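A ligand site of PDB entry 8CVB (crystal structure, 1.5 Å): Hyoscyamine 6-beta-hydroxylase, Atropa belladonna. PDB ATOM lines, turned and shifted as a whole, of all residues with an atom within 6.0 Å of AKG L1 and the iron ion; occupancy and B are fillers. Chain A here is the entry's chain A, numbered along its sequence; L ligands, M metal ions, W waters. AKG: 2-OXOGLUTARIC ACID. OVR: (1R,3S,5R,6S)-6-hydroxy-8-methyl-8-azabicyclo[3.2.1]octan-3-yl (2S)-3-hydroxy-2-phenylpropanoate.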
ATOM      1  N   LEU A 198     -19.551  -8.238  26.763  1.00  0.00           N
ATOM      2  CA  LEU A 198     -18.736  -8.157  27.987  1.00  0.00           C
ATOM      3  C   LEU A 198     -19.362  -7.105  28.898  1.00  0.00           C
ATOM      4  O   LEU A 198     -19.364  -5.914  28.521  1.00  0.00           O
ATOM      5  CB  LEU A 198     -17.290  -7.784  27.609  1.00  0.00           C
ATOM      6  CG  LEU A 198     -16.394  -8.946  27.211  1.00  0.00           C
ATOM      7  CD1 LEU A 198     -16.930  -9.663  25.986  1.00  0.00           C
ATOM      8  CD2 LEU A 198     -14.964  -8.460  26.981  1.00  0.00           C
ATOM      9  N   ASN A 200     -18.708  -5.306  32.182  1.00  0.00           N
ATOM     10  CA  ASN A 200     -17.507  -5.019  32.997  1.00  0.00           C
ATOM     11  C   ASN A 200     -17.935  -4.382  34.318  1.00  0.00           C
ATOM     12  O   ASN A 200     -18.648  -3.380  34.278  1.00  0.00           O
ATOM     13  CB  ASN A 200     -16.555  -4.085  32.267  1.00  0.00           C
ATOM     14  CG  ASN A 200     -16.152  -4.650  30.911  1.00  0.00           C
ATOM     15  OD1 ASN A 200     -15.616  -5.748  30.837  1.00  0.00           O
ATOM     16  ND2 ASN A 200     -16.407  -3.897  29.855  1.00  0.00           N
ATOM     17  N   TYR A 202     -16.353  -2.676  37.705  1.00  0.00           N
ATOM     18  CA  TYR A 202     -15.202  -2.010  38.351  1.00  0.00           C
ATOM     19  C   TYR A 202     -15.604  -1.631  39.762  1.00  0.00           C
ATOM     20  O   TYR A 202     -16.259  -0.601  39.975  1.00  0.00           O
ATOM     21  CB  TYR A 202     -14.779  -0.792  37.522  1.00  0.00           C
ATOM     22  CG  TYR A 202     -14.569  -1.069  36.062  1.00  0.00           C
ATOM     23  CD1 TYR A 202     -13.348  -1.519  35.580  1.00  0.00           C
ATOM     24  CD2 TYR A 202     -15.595  -0.896  35.147  1.00  0.00           C
ATOM     25  CE1 TYR A 202     -13.151  -1.778  34.228  1.00  0.00           C
ATOM     26  CE2 TYR A 202     -15.411  -1.144  33.800  1.00  0.00           C
ATOM     27  CZ  TYR A 202     -14.189  -1.585  33.341  1.00  0.00           C
ATOM     28  OH  TYR A 202     -14.011  -1.826  32.005  1.00  0.00           O
ATOM     29  N   SER A 214      -8.869  -1.306  33.383  1.00  0.00           N
ATOM     30  CA  SER A 214      -8.582  -1.975  32.088  1.00  0.00           C
ATOM     31  C   SER A 214      -7.317  -1.339  31.509  1.00  0.00           C
ATOM     32  O   SER A 214      -7.303  -0.117  31.332  1.00  0.00           O
ATOM     33  CB  SER A 214      -9.764  -1.843  31.158  1.00  0.00           C
ATOM     34  OG  SER A 214      -9.745  -2.854  30.160  1.00  0.00           O
ATOM     35  N   HIS A 217      -5.513  -0.681  25.527  1.00  0.00           N
ATOM     36  CA  HIS A 217      -5.669  -1.721  24.479  1.00  0.00           C
ATOM     37  C   HIS A 217      -6.441  -1.156  23.286  1.00  0.00           C
ATOM     38  O   HIS A 217      -7.286  -0.256  23.484  1.00  0.00           O
ATOM     39  CB  HIS A 217      -6.364  -2.971  25.033  1.00  0.00           C
ATOM     40  CG  HIS A 217      -7.787  -2.736  25.449  1.00  0.00           C
ATOM     41  ND1 HIS A 217      -8.116  -2.124  26.634  1.00  0.00           N
ATOM     42  CD2 HIS A 217      -8.953  -3.010  24.818  1.00  0.00           C
ATOM     43  CE1 HIS A 217      -9.435  -2.041  26.733  1.00  0.00           C
ATOM     44  NE2 HIS A 217      -9.969  -2.588  25.633  1.00  0.00           N
ATOM     45  N   TYR A 218      -6.181  -1.703  22.108  1.00  0.00           N
ATOM     46  CA  TYR A 218      -7.197  -1.822  21.030  1.00  0.00           C
ATOM     47  C   TYR A 218      -8.119  -2.979  21.402  1.00  0.00           C
ATOM     48  O   TYR A 218      -7.629  -3.983  21.963  1.00  0.00           O
ATOM     49  CB  TYR A 218      -6.612  -2.215  19.679  1.00  0.00           C
ATOM     50  CG  TYR A 218      -5.676  -1.236  19.015  1.00  0.00           C
ATOM     51  CD1 TYR A 218      -6.156  -0.183  18.253  1.00  0.00           C
ATOM     52  CD2 TYR A 218      -4.310  -1.417  19.086  1.00  0.00           C
ATOM     53  CE1 TYR A 218      -5.293   0.684  17.614  1.00  0.00           C
ATOM     54  CE2 TYR A 218      -3.432  -0.551  18.447  1.00  0.00           C
ATOM     55  CZ  TYR A 218      -3.927   0.505  17.702  1.00  0.00           C
ATOM     56  OH  TYR A 218      -3.072   1.362  17.065  1.00  0.00           O
ATOM     57  N   ASP A 219      -9.393  -2.876  21.048  1.00  0.00           N
ATOM     58  CA  ASP A 219     -10.262  -4.067  20.918  1.00  0.00           C
ATOM     59  C   ASP A 219      -9.760  -4.820  19.676  1.00  0.00           C
ATOM     60  O   ASP A 219      -9.581  -4.183  18.636  1.00  0.00           O
ATOM     61  CB  ASP A 219     -11.735  -3.686  20.831  1.00  0.00           C
ATOM     62  CG  ASP A 219     -12.320  -3.100  22.115  1.00  0.00           C
ATOM     63  OD1 ASP A 219     -11.619  -3.141  23.158  1.00  0.00           O
ATOM     64  OD2 ASP A 219     -13.465  -2.623  22.068  1.00  0.00           O
ATOM     65  N   THR A 224     -16.641  -2.246  18.235  1.00  0.00           N
ATOM     66  CA  THR A 224     -17.257  -2.417  19.572  1.00  0.00           C
ATOM     67  C   THR A 224     -18.201  -1.254  19.825  1.00  0.00           C
ATOM     68  O   THR A 224     -17.817  -0.108  19.534  1.00  0.00           O
ATOM     69  CB  THR A 224     -16.187  -2.466  20.663  1.00  0.00           C
ATOM     70  OG1 THR A 224     -15.344  -3.587  20.383  1.00  0.00           O
ATOM     71  CG2 THR A 224     -16.781  -2.578  22.053  1.00  0.00           C
ATOM     72  N   LEU A 226     -20.074   0.454  23.067  1.00  0.00           N
ATOM     73  CA  LEU A 226     -19.841   0.488  24.518  1.00  0.00           C
ATOM     74  C   LEU A 226     -20.889   1.409  25.155  1.00  0.00           C
ATOM     75  O   LEU A 226     -21.040   2.549  24.683  1.00  0.00           O
ATOM     76  CB  LEU A 226     -18.410   0.972  24.740  1.00  0.00           C
ATOM     77  CG  LEU A 226     -17.978   1.236  26.174  1.00  0.00           C
ATOM     78  CD1 LEU A 226     -18.087  -0.031  27.015  1.00  0.00           C
ATOM     79  CD2 LEU A 226     -16.558   1.776  26.189  1.00  0.00           C
ATOM     80  N   GLN A 228     -22.036   3.235  28.702  1.00  0.00           N
ATOM     81  CA  GLN A 228     -21.501   3.661  30.020  1.00  0.00           C
ATOM     82  C   GLN A 228     -22.386   4.766  30.608  1.00  0.00           C
ATOM     83  O   GLN A 228     -22.995   5.522  29.823  1.00  0.00           O
ATOM     84  CB  GLN A 228     -20.051   4.140  29.895  1.00  0.00           C
ATOM     85  CG  GLN A 228     -19.879   5.284  28.914  1.00  0.00           C
ATOM     86  CD  GLN A 228     -18.550   5.996  29.053  1.00  0.00           C
ATOM     87  OE1 GLN A 228     -17.743   5.685  29.914  1.00  0.00           O
ATOM     88  NE2 GLN A 228     -18.314   6.952  28.174  1.00  0.00           N
ATOM     89  N   GLY A 232     -14.583   7.118  33.635  1.00  0.00           N
ATOM     90  CA  GLY A 232     -13.507   6.129  33.826  1.00  0.00           C
ATOM     91  C   GLY A 232     -12.853   5.721  32.523  1.00  0.00           C
ATOM     92  O   GLY A 232     -11.692   5.304  32.565  1.00  0.00           O
ATOM     93  N   LEU A 233     -13.588   5.811  31.407  1.00  0.00           N
ATOM     94  CA  LEU A 233     -13.039   5.474  30.069  1.00  0.00           C
ATOM     95  C   LEU A 233     -12.132   6.609  29.600  1.00  0.00           C
ATOM     96  O   LEU A 233     -12.550   7.783  29.657  1.00  0.00           O
ATOM     97  CB  LEU A 233     -14.193   5.246  29.086  1.00  0.00           C
ATOM     98  CG  LEU A 233     -13.778   4.953  27.646  1.00  0.00           C
ATOM     99  CD1 LEU A 233     -12.985   3.651  27.542  1.00  0.00           C
ATOM    100  CD2 LEU A 233     -15.007   4.909  26.747  1.00  0.00           C
ATOM    101  N   ASN A 255     -15.948   2.080  19.287  1.00  0.00           N
ATOM    102  CA  ASN A 255     -14.483   1.834  19.288  1.00  0.00           C
ATOM    103  C   ASN A 255     -14.149   0.998  18.046  1.00  0.00           C
ATOM    104  O   ASN A 255     -14.620  -0.143  17.978  1.00  0.00           O
ATOM    105  CB  ASN A 255     -14.009   1.085  20.542  1.00  0.00           C
ATOM    106  CG  ASN A 255     -13.916   1.955  21.788  1.00  0.00           C
ATOM    107  OD1 ASN A 255     -13.406   3.064  21.726  1.00  0.00           O
ATOM    108  ND2 ASN A 255     -14.351   1.436  22.922  1.00  0.00           N
ATOM    109  N   HIS A 273      -7.720   2.561  24.211  1.00  0.00           N
ATOM    110  CA  HIS A 273      -8.473   3.063  25.380  1.00  0.00           C
ATOM    111  C   HIS A 273      -8.115   2.252  26.626  1.00  0.00           C
ATOM    112  O   HIS A 273      -7.596   1.129  26.502  1.00  0.00           O
ATOM    113  CB  HIS A 273      -9.981   3.078  25.090  1.00  0.00           C
ATOM    114  CG  HIS A 273     -10.499   1.763  24.618  1.00  0.00           C
ATOM    115  ND1 HIS A 273     -10.469   1.386  23.287  1.00  0.00           N
ATOM    116  CD2 HIS A 273     -11.051   0.725  25.294  1.00  0.00           C
ATOM    117  CE1 HIS A 273     -10.985   0.177  23.166  1.00  0.00           C
ATOM    118  NE2 HIS A 273     -11.357  -0.249  24.385  1.00  0.00           N
ATOM    119  N   ARG A 274      -8.399   2.827  27.785  1.00  0.00           N
ATOM    120  CA  ARG A 274      -8.173   2.198  29.109  1.00  0.00           C
ATOM    121  C   ARG A 274      -9.301   2.646  30.043  1.00  0.00           C
ATOM    122  O   ARG A 274     -10.047   3.586  29.683  1.00  0.00           O
ATOM    123  CB  ARG A 274      -6.803   2.593  29.667  1.00  0.00           C
ATOM    124  CG  ARG A 274      -6.749   4.018  30.216  1.00  0.00           C
ATOM    125  CD  ARG A 274      -5.359   4.390  30.672  1.00  0.00           C
ATOM    126  NE  ARG A 274      -5.355   5.753  31.179  1.00  0.00           N
ATOM    127  CZ  ARG A 274      -4.266   6.450  31.475  1.00  0.00           C
ATOM    128  NH1 ARG A 274      -3.069   5.917  31.330  1.00  0.00           N
ATOM    129  NH2 ARG A 274      -4.387   7.691  31.939  1.00  0.00           N
ATOM    130  N   VAL A 275      -9.404   2.001  31.193  1.00  0.00           N
ATOM    131  CA  VAL A 275     -10.379   2.382  32.243  1.00  0.00           C
ATOM    132  C   VAL A 275      -9.614   2.572  33.551  1.00  0.00           C
ATOM    133  O   VAL A 275      -8.842   1.666  33.926  1.00  0.00           O
ATOM    134  CB  VAL A 275     -11.515   1.358  32.383  1.00  0.00           C
ATOM    135  CG1 VAL A 275     -12.513   1.777  33.453  1.00  0.00           C
ATOM    136  CG2 VAL A 275     -12.215   1.124  31.056  1.00  0.00           C
ATOM    137  N   ARG A 283     -18.656   0.916  39.048  1.00  0.00           N
ATOM    138  CA  ARG A 283     -18.987   1.306  37.655  1.00  0.00           C
ATOM    139  C   ARG A 283     -19.274   0.029  36.874  1.00  0.00           C
ATOM    140  O   ARG A 283     -18.509  -0.943  37.029  1.00  0.00           O
ATOM    141  CB  ARG A 283     -17.835   2.100  37.035  1.00  0.00           C
ATOM    142  CG  ARG A 283     -18.037   2.428  35.561  1.00  0.00           C
ATOM    143  CD  ARG A 283     -16.969   3.398  35.077  1.00  0.00           C
ATOM    144  NE  ARG A 283     -17.128   3.741  33.666  1.00  0.00           N
ATOM    145  CZ  ARG A 283     -16.698   3.000  32.654  1.00  0.00           C
ATOM    146  NH1 ARG A 283     -16.079   1.859  32.867  1.00  0.00           N
ATOM    147  NH2 ARG A 283     -16.899   3.409  31.417  1.00  0.00           N
ATOM    148  N   SER A 285     -19.982  -1.137  32.806  1.00  0.00           N
ATOM    149  CA  SER A 285     -20.052  -0.831  31.357  1.00  0.00           C
ATOM    150  C   SER A 285     -20.464  -2.080  30.596  1.00  0.00           C
ATOM    151  O   SER A 285     -20.218  -3.202  31.096  1.00  0.00           O
ATOM    152  CB  SER A 285     -18.763  -0.264  30.830  1.00  0.00           C
ATOM    153  OG  SER A 285     -17.748  -1.257  30.807  1.00  0.00           O
ATOM    154  N   ALA A 287     -19.973  -3.714  26.898  1.00  0.00           N
ATOM    155  CA  ALA A 287     -19.216  -3.696  25.625  1.00  0.00           C
ATOM    156  C   ALA A 287     -19.730  -4.828  24.734  1.00  0.00           C
ATOM    157  O   ALA A 287     -19.703  -5.981  25.177  1.00  0.00           O
ATOM    158  CB  ALA A 287     -17.747  -3.834  25.896  1.00  0.00           C
ATOM    159  N   LEU A 289     -18.684  -6.576  21.510  1.00  0.00           N
ATOM    160  CA  LEU A 289     -17.496  -6.749  20.653  1.00  0.00           C
ATOM    161  C   LEU A 289     -17.904  -7.619  19.457  1.00  0.00           C
ATOM    162  O   LEU A 289     -18.117  -8.827  19.656  1.00  0.00           O
ATOM    163  CB  LEU A 289     -16.367  -7.409  21.456  1.00  0.00           C
ATOM    164  CG  LEU A 289     -15.582  -6.478  22.387  1.00  0.00           C
ATOM    165  CD1 LEU A 289     -16.402  -6.046  23.590  1.00  0.00           C
ATOM    166  CD2 LEU A 289     -14.293  -7.156  22.833  1.00  0.00           C
HETATM  167  C1  AKG L   1     -13.942  -3.270  26.779  1.00  0.00           C
HETATM  168  O1  AKG L   1     -13.203  -3.644  25.850  1.00  0.00           O
HETATM  169  O2  AKG L   1     -14.786  -4.018  27.293  1.00  0.00           O
HETATM  170  C2  AKG L   1     -13.793  -2.046  27.211  1.00  0.00           C
HETATM  171  O5  AKG L   1     -12.874  -1.363  26.749  1.00  0.00           O
HETATM  172  C3  AKG L   1     -14.692  -1.428  28.260  1.00  0.00           C
HETATM  173  C4  AKG L   1     -14.393   0.029  28.563  1.00  0.00           C
HETATM  174  C5  AKG L   1     -15.234   0.650  29.652  1.00  0.00           C
HETATM  175  O3  AKG L   1     -15.679   1.809  29.467  1.00  0.00           O
HETATM  176  O4  AKG L   1     -15.429  -0.001  30.699  1.00  0.00           O
HETATM  177  C1  OVR L   2     -11.227  -7.718  26.999  1.00  0.00           C
HETATM  178  C2  OVR L   2     -10.836  -9.154  26.661  1.00  0.00           C
HETATM  179  C3  OVR L   2      -9.952  -9.242  25.438  1.00  0.00           C
HETATM  180  C4  OVR L   2      -8.965  -8.107  25.323  1.00  0.00           C
HETATM  181  C5  OVR L   2      -9.551  -6.771  25.772  1.00  0.00           C
HETATM  182  C6  OVR L   2     -10.834  -6.325  25.067  1.00  0.00           C
HETATM  183  N1  OVR L   2      -9.979  -6.922  27.172  1.00  0.00           N
HETATM  184  C7  OVR L   2     -11.956  -6.984  25.885  1.00  0.00           C
HETATM  185  O1  OVR L   2     -12.824  -6.011  26.454  1.00  0.00           O
HETATM  186  C8  OVR L   2     -10.150  -5.650  27.888  1.00  0.00           C
HETATM  187  O2  OVR L   2     -10.795  -9.217  24.240  1.00  0.00           O
HETATM  188  C9  OVR L   2     -11.398 -10.367  23.865  1.00  0.00           C
HETATM  189  C10 OVR L   2     -12.095 -10.233  22.532  1.00  0.00           C
HETATM  190  C11 OVR L   2     -11.178 -10.726  21.427  1.00  0.00           C
HETATM  191  C12 OVR L   2     -10.543 -11.961  21.520  1.00  0.00           C
HETATM  192  C13 OVR L   2      -9.721 -12.408  20.498  1.00  0.00           C
HETATM  193  C14 OVR L   2      -9.539 -11.654  19.362  1.00  0.00           C
HETATM  194  C15 OVR L   2     -10.169 -10.434  19.253  1.00  0.00           C
HETATM  195  C16 OVR L   2     -10.982  -9.975  20.274  1.00  0.00           C
HETATM  196  C17 OVR L   2     -13.439 -10.931  22.547  1.00  0.00           C
HETATM  197  O3  OVR L   2     -14.019 -10.869  21.249  1.00  0.00           O
HETATM  198  O4  OVR L   2     -11.388 -11.373  24.517  1.00  0.00           O
HETATM  199 FE    FE M   1     -11.974  -2.191  24.975  1.00  0.00          FE
HETATM  200  O   HOH W   1     -13.281  -6.062  29.352  1.00  0.00           O
HETATM  201  O   HOH W   2     -14.239  -1.243  24.106  1.00  0.00           O
HETATM  202  O   HOH W   3     -12.380  -3.397  30.073  1.00  0.00           O
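Three residues have an atom within 4 Å of the iron ion: His 217, Asp 219 and His 273.
The nearest printed residue that does not touch the iron ion is Asn 255 (4.8 Å).
N of Asn 200 lies within hydrogen-bond range of O of Ser 285 (2.8 Å).
The side-chain hydroxyl of Thr 224 lies within hydrogen-bond range of the side-chain carboxylate of Asp 219.
The backbone carbonyl oxygen of Ala 287 lies within hydrogen-bond range of the backbone NH of Leu 198 (2.8 Å).
The guanidinium group (NH2) of Arg 283 sits at hydrogen-bond distance from the side-chain amide oxygen (OE1) of Gln 228 (2.9 Å).
N of Val 275 is in hydrogen-bond range of O of Ser 214, at 3.0 Å.
The backbone NH (N) of Tyr 202 sits at hydrogen-bond distance from the backbone carbonyl oxygen (O) of Arg 283, at 2.8 Å.
The side-chain carboxylate (OD1) of Asp 219 binds the iron ion, 2.1 Å away.
O1 of AKG L1 is bound to the iron ion.
A ring nitrogen (NE2) of His 273 is bound to the iron ion (2.1 Å).
NE2 of His 217 is bound to the iron ion (2.1 Å).
O5 of AKG L1 binds the iron ion (2.2 Å).
Slightly farther from the iron ion lies water W2 (2.6 Å).
An oxygen (O4) of AKG L1 lies within hydrogen-bond range of the side-chain hydroxyl of Ser 285 (2.6 Å).
O4 of AKG L1 is in hydrogen-bond range of OH of Tyr 202 (2.7 Å).
An oxygen (O2) of AKG L1 sits at hydrogen-bond distance from the side-chain amide nitrogen of Asn 200, 3.0 Å away.
The guanidinium group of Arg 283 lies within salt-bridge range of an oxygen (O3) of AKG L1 (2.8 Å).
Merely in contact with AKG L1: Leu 226, Leu 233, Val 275 and Ala 287.
Of the 20 residues printed, 11 come within 4 Å of AKG L1.
Water W2 lies within hydrogen-bond range of OD2 of Asp 219 and ND2 of Asn 255.
Water W1 lies within hydrogen-bond range of OD1 of Asn 200 (2.8 Å), O1 of OVR L2 (2.9 Å) and O2 of AKG L1 (3.3 Å).
Water W3 lies within hydrogen-bond range of the side-chain hydroxyl of Ser 214 (2.7 Å) and the side-chain hydroxyl of Tyr 202 (3.0 Å).
An oxygen (O2) of AKG L1 is in hydrogen-bond range of an oxygen (O1) of OVR L2 (2.9 Å).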
